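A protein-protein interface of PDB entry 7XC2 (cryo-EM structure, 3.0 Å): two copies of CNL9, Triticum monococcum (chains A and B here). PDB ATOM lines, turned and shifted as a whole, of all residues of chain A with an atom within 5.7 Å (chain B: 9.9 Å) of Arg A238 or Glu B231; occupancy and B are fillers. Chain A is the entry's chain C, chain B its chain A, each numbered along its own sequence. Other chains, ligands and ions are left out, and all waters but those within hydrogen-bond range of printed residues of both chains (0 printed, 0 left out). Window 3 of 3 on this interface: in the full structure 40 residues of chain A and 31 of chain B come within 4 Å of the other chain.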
ATOM      1  N   LYS A 215       6.511   7.520  27.086  1.00  0.00           N
ATOM      2  CA  LYS A 215       6.559   8.014  25.718  1.00  0.00           C
ATOM      3  C   LYS A 215       5.258   8.699  25.339  1.00  0.00           C
ATOM      4  O   LYS A 215       5.268   9.760  24.708  1.00  0.00           O
ATOM      5  CB  LYS A 215       6.847   6.870  24.758  1.00  0.00           C
ATOM      6  CG  LYS A 215       8.258   6.367  24.798  1.00  0.00           C
ATOM      7  CD  LYS A 215       8.450   5.304  23.750  1.00  0.00           C
ATOM      8  CE  LYS A 215       9.845   4.744  23.785  1.00  0.00           C
ATOM      9  NZ  LYS A 215      10.030   3.707  22.740  1.00  0.00           N
ATOM     10  N   ILE A 233       3.887  13.713  15.614  1.00  0.00           N
ATOM     11  CA  ILE A 233       4.822  13.273  16.633  1.00  0.00           C
ATOM     12  C   ILE A 233       4.417  11.944  17.238  1.00  0.00           C
ATOM     13  O   ILE A 233       5.267  11.226  17.766  1.00  0.00           O
ATOM     14  CB  ILE A 233       4.956  14.356  17.714  1.00  0.00           C
ATOM     15  CG1 ILE A 233       6.091  14.025  18.671  1.00  0.00           C
ATOM     16  CG2 ILE A 233       3.675  14.496  18.468  1.00  0.00           C
ATOM     17  CD1 ILE A 233       7.435  14.087  18.039  1.00  0.00           C
ATOM     18  N   ALA A 236       6.458   9.018  15.648  1.00  0.00           N
ATOM     19  CA  ALA A 236       7.900   8.927  15.799  1.00  0.00           C
ATOM     20  C   ALA A 236       8.262   7.820  16.774  1.00  0.00           C
ATOM     21  O   ALA A 236       7.493   7.483  17.673  1.00  0.00           O
ATOM     22  CB  ALA A 236       8.467  10.252  16.288  1.00  0.00           C
ATOM     23  N   ALA A 237       9.448   7.242  16.591  1.00  0.00           N
ATOM     24  CA  ALA A 237       9.917   6.154  17.446  1.00  0.00           C
ATOM     25  C   ALA A 237      11.319   6.474  17.948  1.00  0.00           C
ATOM     26  O   ALA A 237      12.296   5.924  17.455  1.00  0.00           O
ATOM     27  CB  ALA A 237       9.885   4.840  16.694  1.00  0.00           C
ATOM     28  N   ARG A 238      11.407   7.314  18.968  1.00  0.00           N
ATOM     29  CA  ARG A 238      12.651   7.619  19.658  1.00  0.00           C
ATOM     30  C   ARG A 238      12.478   7.303  21.135  1.00  0.00           C
ATOM     31  O   ARG A 238      11.362   7.139  21.622  1.00  0.00           O
ATOM     32  CB  ARG A 238      13.046   9.082  19.479  1.00  0.00           C
ATOM     33  CG  ARG A 238      12.666   9.684  18.169  1.00  0.00           C
ATOM     34  CD  ARG A 238      12.732  11.185  18.265  1.00  0.00           C
ATOM     35  NE  ARG A 238      12.055  11.825  17.150  1.00  0.00           N
ATOM     36  CZ  ARG A 238      11.737  13.111  17.110  1.00  0.00           C
ATOM     37  NH1 ARG A 238      12.030  13.901  18.127  1.00  0.00           N
ATOM     38  NH2 ARG A 238      11.123  13.603  16.050  1.00  0.00           N
ATOM     39  N   ASP A 239      13.581   7.231  21.866  1.00  0.00           N
ATOM     40  CA  ASP A 239      13.450   6.951  23.284  1.00  0.00           C
ATOM     41  C   ASP A 239      13.093   8.222  24.043  1.00  0.00           C
ATOM     42  O   ASP A 239      12.899   9.291  23.466  1.00  0.00           O
ATOM     43  CB  ASP A 239      14.721   6.323  23.843  1.00  0.00           C
ATOM     44  CG  ASP A 239      15.950   7.150  23.570  1.00  0.00           C
ATOM     45  OD1 ASP A 239      15.915   8.380  23.764  1.00  0.00           O
ATOM     46  OD2 ASP A 239      16.986   6.558  23.214  1.00  0.00           O
ATOM     47  N   GLU A 240      13.024   8.104  25.366  1.00  0.00           N
ATOM     48  CA  GLU A 240      12.603   9.233  26.181  1.00  0.00           C
ATOM     49  C   GLU A 240      13.619  10.361  26.174  1.00  0.00           C
ATOM     50  O   GLU A 240      13.234  11.527  26.291  1.00  0.00           O
ATOM     51  CB  GLU A 240      12.354   8.780  27.613  1.00  0.00           C
ATOM     52  CG  GLU A 240      11.149   7.902  27.784  1.00  0.00           C
ATOM     53  CD  GLU A 240      11.445   6.448  27.538  1.00  0.00           C
ATOM     54  OE1 GLU A 240      12.479   6.146  26.912  1.00  0.00           O
ATOM     55  OE2 GLU A 240      10.643   5.600  27.975  1.00  0.00           O
ATOM     56  N   TYR A 242      15.463  11.664  23.814  1.00  0.00           N
ATOM     57  CA  TYR A 242      15.346  12.599  22.706  1.00  0.00           C
ATOM     58  C   TYR A 242      14.054  13.395  22.773  1.00  0.00           C
ATOM     59  O   TYR A 242      14.037  14.575  22.409  1.00  0.00           O
ATOM     60  CB  TYR A 242      15.465  11.848  21.392  1.00  0.00           C
ATOM     61  CG  TYR A 242      16.854  11.327  21.181  1.00  0.00           C
ATOM     62  CD1 TYR A 242      17.913  12.196  21.022  1.00  0.00           C
ATOM     63  CD2 TYR A 242      17.115   9.974  21.160  1.00  0.00           C
ATOM     64  CE1 TYR A 242      19.182  11.738  20.839  1.00  0.00           C
ATOM     65  CE2 TYR A 242      18.387   9.505  20.977  1.00  0.00           C
ATOM     66  CZ  TYR A 242      19.415  10.393  20.817  1.00  0.00           C
ATOM     67  OH  TYR A 242      20.693   9.941  20.634  1.00  0.00           O
ATOM     68  N   LEU A 243      12.973  12.791  23.257  1.00  0.00           N
ATOM     69  CA  LEU A 243      11.745  13.550  23.448  1.00  0.00           C
ATOM     70  C   LEU A 243      11.930  14.632  24.502  1.00  0.00           C
ATOM     71  O   LEU A 243      11.459  15.764  24.335  1.00  0.00           O
ATOM     72  CB  LEU A 243      10.611  12.608  23.831  1.00  0.00           C
ATOM     73  CG  LEU A 243      10.276  11.555  22.786  1.00  0.00           C
ATOM     74  CD1 LEU A 243       9.291  10.565  23.336  1.00  0.00           C
ATOM     75  CD2 LEU A 243       9.718  12.212  21.562  1.00  0.00           C
ATOM     76  N   ASP A 246      13.781  17.451  22.969  1.00  0.00           N
ATOM     77  CA  ASP A 246      12.913  18.270  22.131  1.00  0.00           C
ATOM     78  C   ASP A 246      12.090  19.232  22.970  1.00  0.00           C
ATOM     79  O   ASP A 246      11.974  20.419  22.639  1.00  0.00           O
ATOM     80  CB  ASP A 246      11.993  17.385  21.300  1.00  0.00           C
ATOM     81  CG  ASP A 246      12.747  16.523  20.326  1.00  0.00           C
ATOM     82  OD1 ASP A 246      13.990  16.504  20.397  1.00  0.00           O
ATOM     83  OD2 ASP A 246      12.103  15.864  19.485  1.00  0.00           O
ATOM     84  N   MET B 137      19.285   7.596  33.812  1.00  0.00           N
ATOM     85  CA  MET B 137      18.996   8.602  32.804  1.00  0.00           C
ATOM     86  C   MET B 137      18.782   9.970  33.427  1.00  0.00           C
ATOM     87  O   MET B 137      19.182  10.983  32.847  1.00  0.00           O
ATOM     88  CB  MET B 137      17.772   8.200  31.993  1.00  0.00           C
ATOM     89  CG  MET B 137      17.565   9.039  30.761  1.00  0.00           C
ATOM     90  SD  MET B 137      15.931   8.802  30.070  1.00  0.00           S
ATOM     91  CE  MET B 137      14.953   9.603  31.325  1.00  0.00           C
ATOM     92  N   LYS B 216      19.442   0.256  16.609  1.00  0.00           N
ATOM     93  CA  LYS B 216      19.093   1.400  17.437  1.00  0.00           C
ATOM     94  C   LYS B 216      20.302   2.285  17.686  1.00  0.00           C
ATOM     95  O   LYS B 216      20.196   3.512  17.650  1.00  0.00           O
ATOM     96  CB  LYS B 216      18.494   0.924  18.752  1.00  0.00           C
ATOM     97  CG  LYS B 216      17.931   2.023  19.611  1.00  0.00           C
ATOM     98  CD  LYS B 216      17.279   1.438  20.846  1.00  0.00           C
ATOM     99  CE  LYS B 216      16.791   2.516  21.789  1.00  0.00           C
ATOM    100  NZ  LYS B 216      17.909   3.339  22.313  1.00  0.00           N
ATOM    101  N   LYS B 219      21.094   4.237  14.453  1.00  0.00           N
ATOM    102  CA  LYS B 219      20.110   5.291  14.254  1.00  0.00           C
ATOM    103  C   LYS B 219      20.320   6.428  15.241  1.00  0.00           C
ATOM    104  O   LYS B 219      20.131   7.597  14.897  1.00  0.00           O
ATOM    105  CB  LYS B 219      18.706   4.723  14.386  1.00  0.00           C
ATOM    106  CG  LYS B 219      18.308   3.805  13.269  1.00  0.00           C
ATOM    107  CD  LYS B 219      17.074   3.036  13.645  1.00  0.00           C
ATOM    108  CE  LYS B 219      16.582   2.192  12.505  1.00  0.00           C
ATOM    109  NZ  LYS B 219      15.463   1.329  12.939  1.00  0.00           N
ATOM    110  N   ASP B 220      20.709   6.105  16.473  1.00  0.00           N
ATOM    111  CA  ASP B 220      20.987   7.146  17.453  1.00  0.00           C
ATOM    112  C   ASP B 220      22.146   8.019  17.010  1.00  0.00           C
ATOM    113  O   ASP B 220      22.078   9.247  17.110  1.00  0.00           O
ATOM    114  CB  ASP B 220      21.289   6.522  18.807  1.00  0.00           C
ATOM    115  CG  ASP B 220      20.044   6.111  19.545  1.00  0.00           C
ATOM    116  OD1 ASP B 220      18.943   6.368  19.029  1.00  0.00           O
ATOM    117  OD2 ASP B 220      20.161   5.533  20.642  1.00  0.00           O
ATOM    118  N   LEU B 222      23.169   8.555  13.944  1.00  0.00           N
ATOM    119  CA  LEU B 222      22.753   9.353  12.797  1.00  0.00           C
ATOM    120  C   LEU B 222      21.886  10.525  13.225  1.00  0.00           C
ATOM    121  O   LEU B 222      22.090  11.657  12.781  1.00  0.00           O
ATOM    122  CB  LEU B 222      22.015   8.476  11.795  1.00  0.00           C
ATOM    123  CG  LEU B 222      22.899   7.835  10.741  1.00  0.00           C
ATOM    124  CD1 LEU B 222      22.084   6.918   9.891  1.00  0.00           C
ATOM    125  CD2 LEU B 222      23.524   8.905   9.903  1.00  0.00           C
ATOM    126  N   TYR B 223      20.910  10.276  14.095  1.00  0.00           N
ATOM    127  CA  TYR B 223      20.026  11.347  14.530  1.00  0.00           C
ATOM    128  C   TYR B 223      20.762  12.381  15.358  1.00  0.00           C
ATOM    129  O   TYR B 223      20.386  13.554  15.353  1.00  0.00           O
ATOM    130  CB  TYR B 223      18.861  10.773  15.326  1.00  0.00           C
ATOM    131  CG  TYR B 223      17.922  11.807  15.879  1.00  0.00           C
ATOM    132  CD1 TYR B 223      16.921  12.344  15.100  1.00  0.00           C
ATOM    133  CD2 TYR B 223      18.025  12.233  17.183  1.00  0.00           C
ATOM    134  CE1 TYR B 223      16.062  13.279  15.600  1.00  0.00           C
ATOM    135  CE2 TYR B 223      17.170  13.168  17.689  1.00  0.00           C
ATOM    136  CZ  TYR B 223      16.191  13.686  16.893  1.00  0.00           C
ATOM    137  OH  TYR B 223      15.334  14.621  17.401  1.00  0.00           O
ATOM    138  N   GLY B 224      21.804  11.974  16.079  1.00  0.00           N
ATOM    139  CA  GLY B 224      22.578  12.941  16.829  1.00  0.00           C
ATOM    140  C   GLY B 224      23.459  13.804  15.955  1.00  0.00           C
ATOM    141  O   GLY B 224      23.745  14.949  16.300  1.00  0.00           O
ATOM    142  N   LEU B 225      23.900  13.276  14.814  1.00  0.00           N
ATOM    143  CA  LEU B 225      24.790  14.056  13.963  1.00  0.00           C
ATOM    144  C   LEU B 225      24.060  15.206  13.284  1.00  0.00           C
ATOM    145  O   LEU B 225      24.628  16.288  13.118  1.00  0.00           O
ATOM    146  CB  LEU B 225      25.448  13.157  12.927  1.00  0.00           C
ATOM    147  CG  LEU B 225      26.618  12.340  13.454  1.00  0.00           C
ATOM    148  CD1 LEU B 225      27.013  11.293  12.453  1.00  0.00           C
ATOM    149  CD2 LEU B 225      27.776  13.248  13.748  1.00  0.00           C
ATOM    150  N   ASP B 226      22.809  14.998  12.879  1.00  0.00           N
ATOM    151  CA  ASP B 226      22.044  16.053  12.215  1.00  0.00           C
ATOM    152  C   ASP B 226      20.560  15.816  12.458  1.00  0.00           C
ATOM    153  O   ASP B 226      19.972  14.925  11.847  1.00  0.00           O
ATOM    154  CB  ASP B 226      22.345  16.090  10.726  1.00  0.00           C
ATOM    155  CG  ASP B 226      21.732  17.285  10.044  1.00  0.00           C
ATOM    156  OD1 ASP B 226      21.089  18.097  10.734  1.00  0.00           O
ATOM    157  OD2 ASP B 226      21.893  17.420   8.817  1.00  0.00           O
ATOM    158  N   LYS B 227      19.953  16.636  13.315  1.00  0.00           N
ATOM    159  CA  LYS B 227      18.559  16.434  13.682  1.00  0.00           C
ATOM    160  C   LYS B 227      17.595  16.764  12.558  1.00  0.00           C
ATOM    161  O   LYS B 227      16.454  16.303  12.590  1.00  0.00           O
ATOM    162  CB  LYS B 227      18.197  17.282  14.895  1.00  0.00           C
ATOM    163  CG  LYS B 227      18.689  16.740  16.207  1.00  0.00           C
ATOM    164  CD  LYS B 227      18.072  17.495  17.365  1.00  0.00           C
ATOM    165  CE  LYS B 227      18.463  16.871  18.693  1.00  0.00           C
ATOM    166  NZ  LYS B 227      17.618  17.357  19.819  1.00  0.00           N
ATOM    167  N   VAL B 228      18.005  17.563  11.582  1.00  0.00           N
ATOM    168  CA  VAL B 228      17.089  17.993  10.533  1.00  0.00           C
ATOM    169  C   VAL B 228      17.065  17.009   9.377  1.00  0.00           C
ATOM    170  O   VAL B 228      16.002  16.539   8.972  1.00  0.00           O
ATOM    171  CB  VAL B 228      17.465  19.406  10.056  1.00  0.00           C
ATOM    172  CG1 VAL B 228      16.686  19.754   8.820  1.00  0.00           C
ATOM    173  CG2 VAL B 228      17.191  20.407  11.146  1.00  0.00           C
ATOM    174  N   LYS B 229      18.234  16.687   8.827  1.00  0.00           N
ATOM    175  CA  LYS B 229      18.296  15.773   7.695  1.00  0.00           C
ATOM    176  C   LYS B 229      17.762  14.400   8.067  1.00  0.00           C
ATOM    177  O   LYS B 229      16.835  13.887   7.435  1.00  0.00           O
ATOM    178  CB  LYS B 229      19.731  15.675   7.193  1.00  0.00           C
ATOM    179  CG  LYS B 229      19.908  14.751   6.021  1.00  0.00           C
ATOM    180  CD  LYS B 229      21.334  14.793   5.525  1.00  0.00           C
ATOM    181  CE  LYS B 229      21.577  13.735   4.476  1.00  0.00           C
ATOM    182  NZ  LYS B 229      20.789  13.995   3.250  1.00  0.00           N
ATOM    183  N   TYR B 230      18.339  13.783   9.090  1.00  0.00           N
ATOM    184  CA  TYR B 230      17.906  12.461   9.530  1.00  0.00           C
ATOM    185  C   TYR B 230      16.877  12.549  10.642  1.00  0.00           C
ATOM    186  O   TYR B 230      16.981  11.876  11.659  1.00  0.00           O
ATOM    187  CB  TYR B 230      19.110  11.647   9.974  1.00  0.00           C
ATOM    188  CG  TYR B 230      20.154  11.520   8.910  1.00  0.00           C
ATOM    189  CD1 TYR B 230      19.988  10.641   7.864  1.00  0.00           C
ATOM    190  CD2 TYR B 230      21.298  12.283   8.947  1.00  0.00           C
ATOM    191  CE1 TYR B 230      20.930  10.524   6.888  1.00  0.00           C
ATOM    192  CE2 TYR B 230      22.246  12.173   7.976  1.00  0.00           C
ATOM    193  CZ  TYR B 230      22.057  11.293   6.948  1.00  0.00           C
ATOM    194  OH  TYR B 230      23.006  11.175   5.967  1.00  0.00           O
ATOM    195  N   GLU B 231      15.849  13.363  10.439  1.00  0.00           N
ATOM    196  CA  GLU B 231      14.886  13.593  11.506  1.00  0.00           C
ATOM    197  C   GLU B 231      13.997  12.381  11.723  1.00  0.00           C
ATOM    198  O   GLU B 231      13.598  12.092  12.854  1.00  0.00           O
ATOM    199  CB  GLU B 231      14.047  14.821  11.186  1.00  0.00           C
ATOM    200  CG  GLU B 231      13.137  15.234  12.302  1.00  0.00           C
ATOM    201  CD  GLU B 231      11.741  14.710  12.112  1.00  0.00           C
ATOM    202  OE1 GLU B 231      11.411  14.324  10.973  1.00  0.00           O
ATOM    203  OE2 GLU B 231      10.974  14.678  13.097  1.00  0.00           O
ATOM    204  N   ASN B 232      13.674  11.660  10.659  1.00  0.00           N
ATOM    205  CA  ASN B 232      12.777  10.519  10.738  1.00  0.00           C
ATOM    206  C   ASN B 232      13.525   9.200  10.603  1.00  0.00           C
ATOM    207  O   ASN B 232      12.949   8.186  10.216  1.00  0.00           O
ATOM    208  CB  ASN B 232      11.695  10.636   9.672  1.00  0.00           C
ATOM    209  CG  ASN B 232      10.486   9.808   9.989  1.00  0.00           C
ATOM    210  OD1 ASN B 232       9.821  10.027  10.996  1.00  0.00           O
ATOM    211  ND2 ASN B 232      10.185   8.848   9.130  1.00  0.00           N
ATOM    212  N   ILE B 233      14.815   9.200  10.938  1.00  0.00           N
ATOM    213  CA  ILE B 233      15.641   8.029  10.707  1.00  0.00           C
ATOM    214  C   ILE B 233      15.226   6.861  11.580  1.00  0.00           C
ATOM    215  O   ILE B 233      15.494   5.711  11.232  1.00  0.00           O
ATOM    216  CB  ILE B 233      17.118   8.386  10.927  1.00  0.00           C
ATOM    217  CG1 ILE B 233      18.022   7.248  10.476  1.00  0.00           C
ATOM    218  CG2 ILE B 233      17.367   8.698  12.366  1.00  0.00           C
ATOM    219  CD1 ILE B 233      18.000   7.022   9.006  1.00  0.00           C
ATOM    220  N   HIS B 234      14.557   7.112  12.697  1.00  0.00           N
ATOM    221  CA  HIS B 234      14.196   6.007  13.570  1.00  0.00           C
ATOM    222  C   HIS B 234      13.077   5.152  13.007  1.00  0.00           C
ATOM    223  O   HIS B 234      12.818   4.077  13.551  1.00  0.00           O
ATOM    224  CB  HIS B 234      13.794   6.531  14.937  1.00  0.00           C
ATOM    225  CG  HIS B 234      14.936   7.052  15.745  1.00  0.00           C
ATOM    226  ND1 HIS B 234      15.642   6.267  16.626  1.00  0.00           N
ATOM    227  CD2 HIS B 234      15.488   8.284  15.813  1.00  0.00           C
ATOM    228  CE1 HIS B 234      16.585   6.991  17.198  1.00  0.00           C
ATOM    229  NE2 HIS B 234      16.513   8.218  16.723  1.00  0.00           N
ATOM    230  N   ASN B 235      12.413   5.591  11.944  1.00  0.00           N
ATOM    231  CA  ASN B 235      11.361   4.808  11.320  1.00  0.00           C
ATOM    232  C   ASN B 235      11.832   4.039  10.098  1.00  0.00           C
ATOM    233  O   ASN B 235      11.110   3.157   9.631  1.00  0.00           O
ATOM    234  CB  ASN B 235      10.194   5.706  10.916  1.00  0.00           C
ATOM    235  CG  ASN B 235       9.309   6.054  12.076  1.00  0.00           C
ATOM    236  OD1 ASN B 235       8.613   5.202  12.612  1.00  0.00           O
ATOM    237  ND2 ASN B 235       9.318   7.315  12.465  1.00  0.00           N
ATOM    238  N   ALA B 236      13.010   4.349   9.570  1.00  0.00           N
ATOM    239  CA  ALA B 236      13.530   3.625   8.424  1.00  0.00           C
ATOM    240  C   ALA B 236      13.765   2.166   8.780  1.00  0.00           C
ATOM    241  O   ALA B 236      14.018   1.824   9.933  1.00  0.00           O
ATOM    242  CB  ALA B 236      14.830   4.255   7.944  1.00  0.00           C
ATOM    243  N   ARG B 238      16.150  -0.459   7.236  1.00  0.00           N
ATOM    244  CA  ARG B 238      17.242  -1.013   6.452  1.00  0.00           C
ATOM    245  C   ARG B 238      18.136  -1.828   7.371  1.00  0.00           C
ATOM    246  O   ARG B 238      18.062  -1.716   8.592  1.00  0.00           O
ATOM    247  CB  ARG B 238      18.055   0.085   5.771  1.00  0.00           C
ATOM    248  CG  ARG B 238      17.275   1.285   5.357  1.00  0.00           C
ATOM    249  CD  ARG B 238      18.214   2.430   5.084  1.00  0.00           C
ATOM    250  NE  ARG B 238      17.509   3.698   5.012  1.00  0.00           N
ATOM    251  CZ  ARG B 238      18.102   4.882   5.040  1.00  0.00           C
ATOM    252  NH1 ARG B 238      19.418   4.966   5.144  1.00  0.00           N
ATOM    253  NH2 ARG B 238      17.377   5.983   4.967  1.00  0.00           N
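3 positions are printed for both chains.
Of the 10 printed residues of chain A, 6 touch a printed residue of chain B. Printed residues of chain A that touch a printed residue of chain B: Ala A236, Ala A237, Arg A238, Asp A239, Tyr A242 and Asp A246. Of the 20 printed residues of chain B, 7 touch a printed residue of chain A. Printed residues of chain B that touch a printed residue of chain A: Lys B216, Asp B220, Tyr B223, Lys B227, Glu B231, His B234 and Asn B235. Hydrophobic or aromatic side chains of chain B within 4 Å of the printed part of chain A: Tyr B223 and His B234. Among the printed residues, 10 pairs touch across the chains. Among the printed residues, Asp or Glu carboxylates within 4 Å of a Lys or Arg side-chain nitrogen of the other chain: Arg A238 with Glu B231, Asp A239 with Lys B216 and Asp A246 with Lys B227.
The side-chain amide oxygen (OD1) of Asn B232 sits at hydrogen-bond distance from the side-chain amide nitrogen (ND2) of Asn B235 (3.1 Å). N of Tyr A242 sits close to OD1 of Asp A239 (3.3 Å). The guanidinium group (NH1) of Arg A238 lies within salt-bridge range of the side-chain carboxylate (OD1) of Asp A246 (3.97 Å). NZ of Lys B216 lies within salt-bridge range of OD2 of Asp B220 (3.6 Å).
Arg A238 touches just these residues of chain B: Tyr B223, Glu B231 and His B234. Glu B231 touches just one residue of chain A: Arg A238. Of chain B, only His B234 (3.0 Å) comes within 4 Å of Ala A237. Asp A239 touches one residue of chain B. Printed residues of chain A within 4 Å of Asn B235: Ala A236. Printed residues of chain A within 4 Å of Asp B220: Tyr A242 (3.7 Å). Printed residues of chain A within 4 Å of Lys B216: Asp A239. Leu B222 touches none of the printed residues of chain A. The nearest residue of chain B that does not touch Arg A238 is Asn B232 (6.3 Å). The nearest printed residue of chain A that does not touch Glu B231 is Ala A236 (6.0 Å). The nearest printed residue of chain A that does not touch His B234 is Tyr A242 (4.8 Å).
Among the printed residues, merely in contact across the chains: Tyr A242 with Tyr B223, Tyr A242 with Asp B220, Asp A246 with Tyr B223, Arg A238 with His B234 and Ala A236 with Asn B235.
A ring nitrogen (ND1) of His B234 lies close to the backbone carbonyl oxygen (O) of Ala A237, 3.5 Å away. The side-chain carboxylate (OD2) of Asp A239 lies within salt-bridge range of the side-chain amino group (NZ) of Lys B216 (3.5 Å). OE2 of Glu B231 lies within salt-bridge range of NH2 of Arg A238. NZ of Lys B227 is in salt-bridge range of OD1 of Asp A246 (3.8 Å). The guanidinium group of Arg A238 is in hydrogen-bond range of the side-chain hydroxyl of Tyr B223 (3.5 Å).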
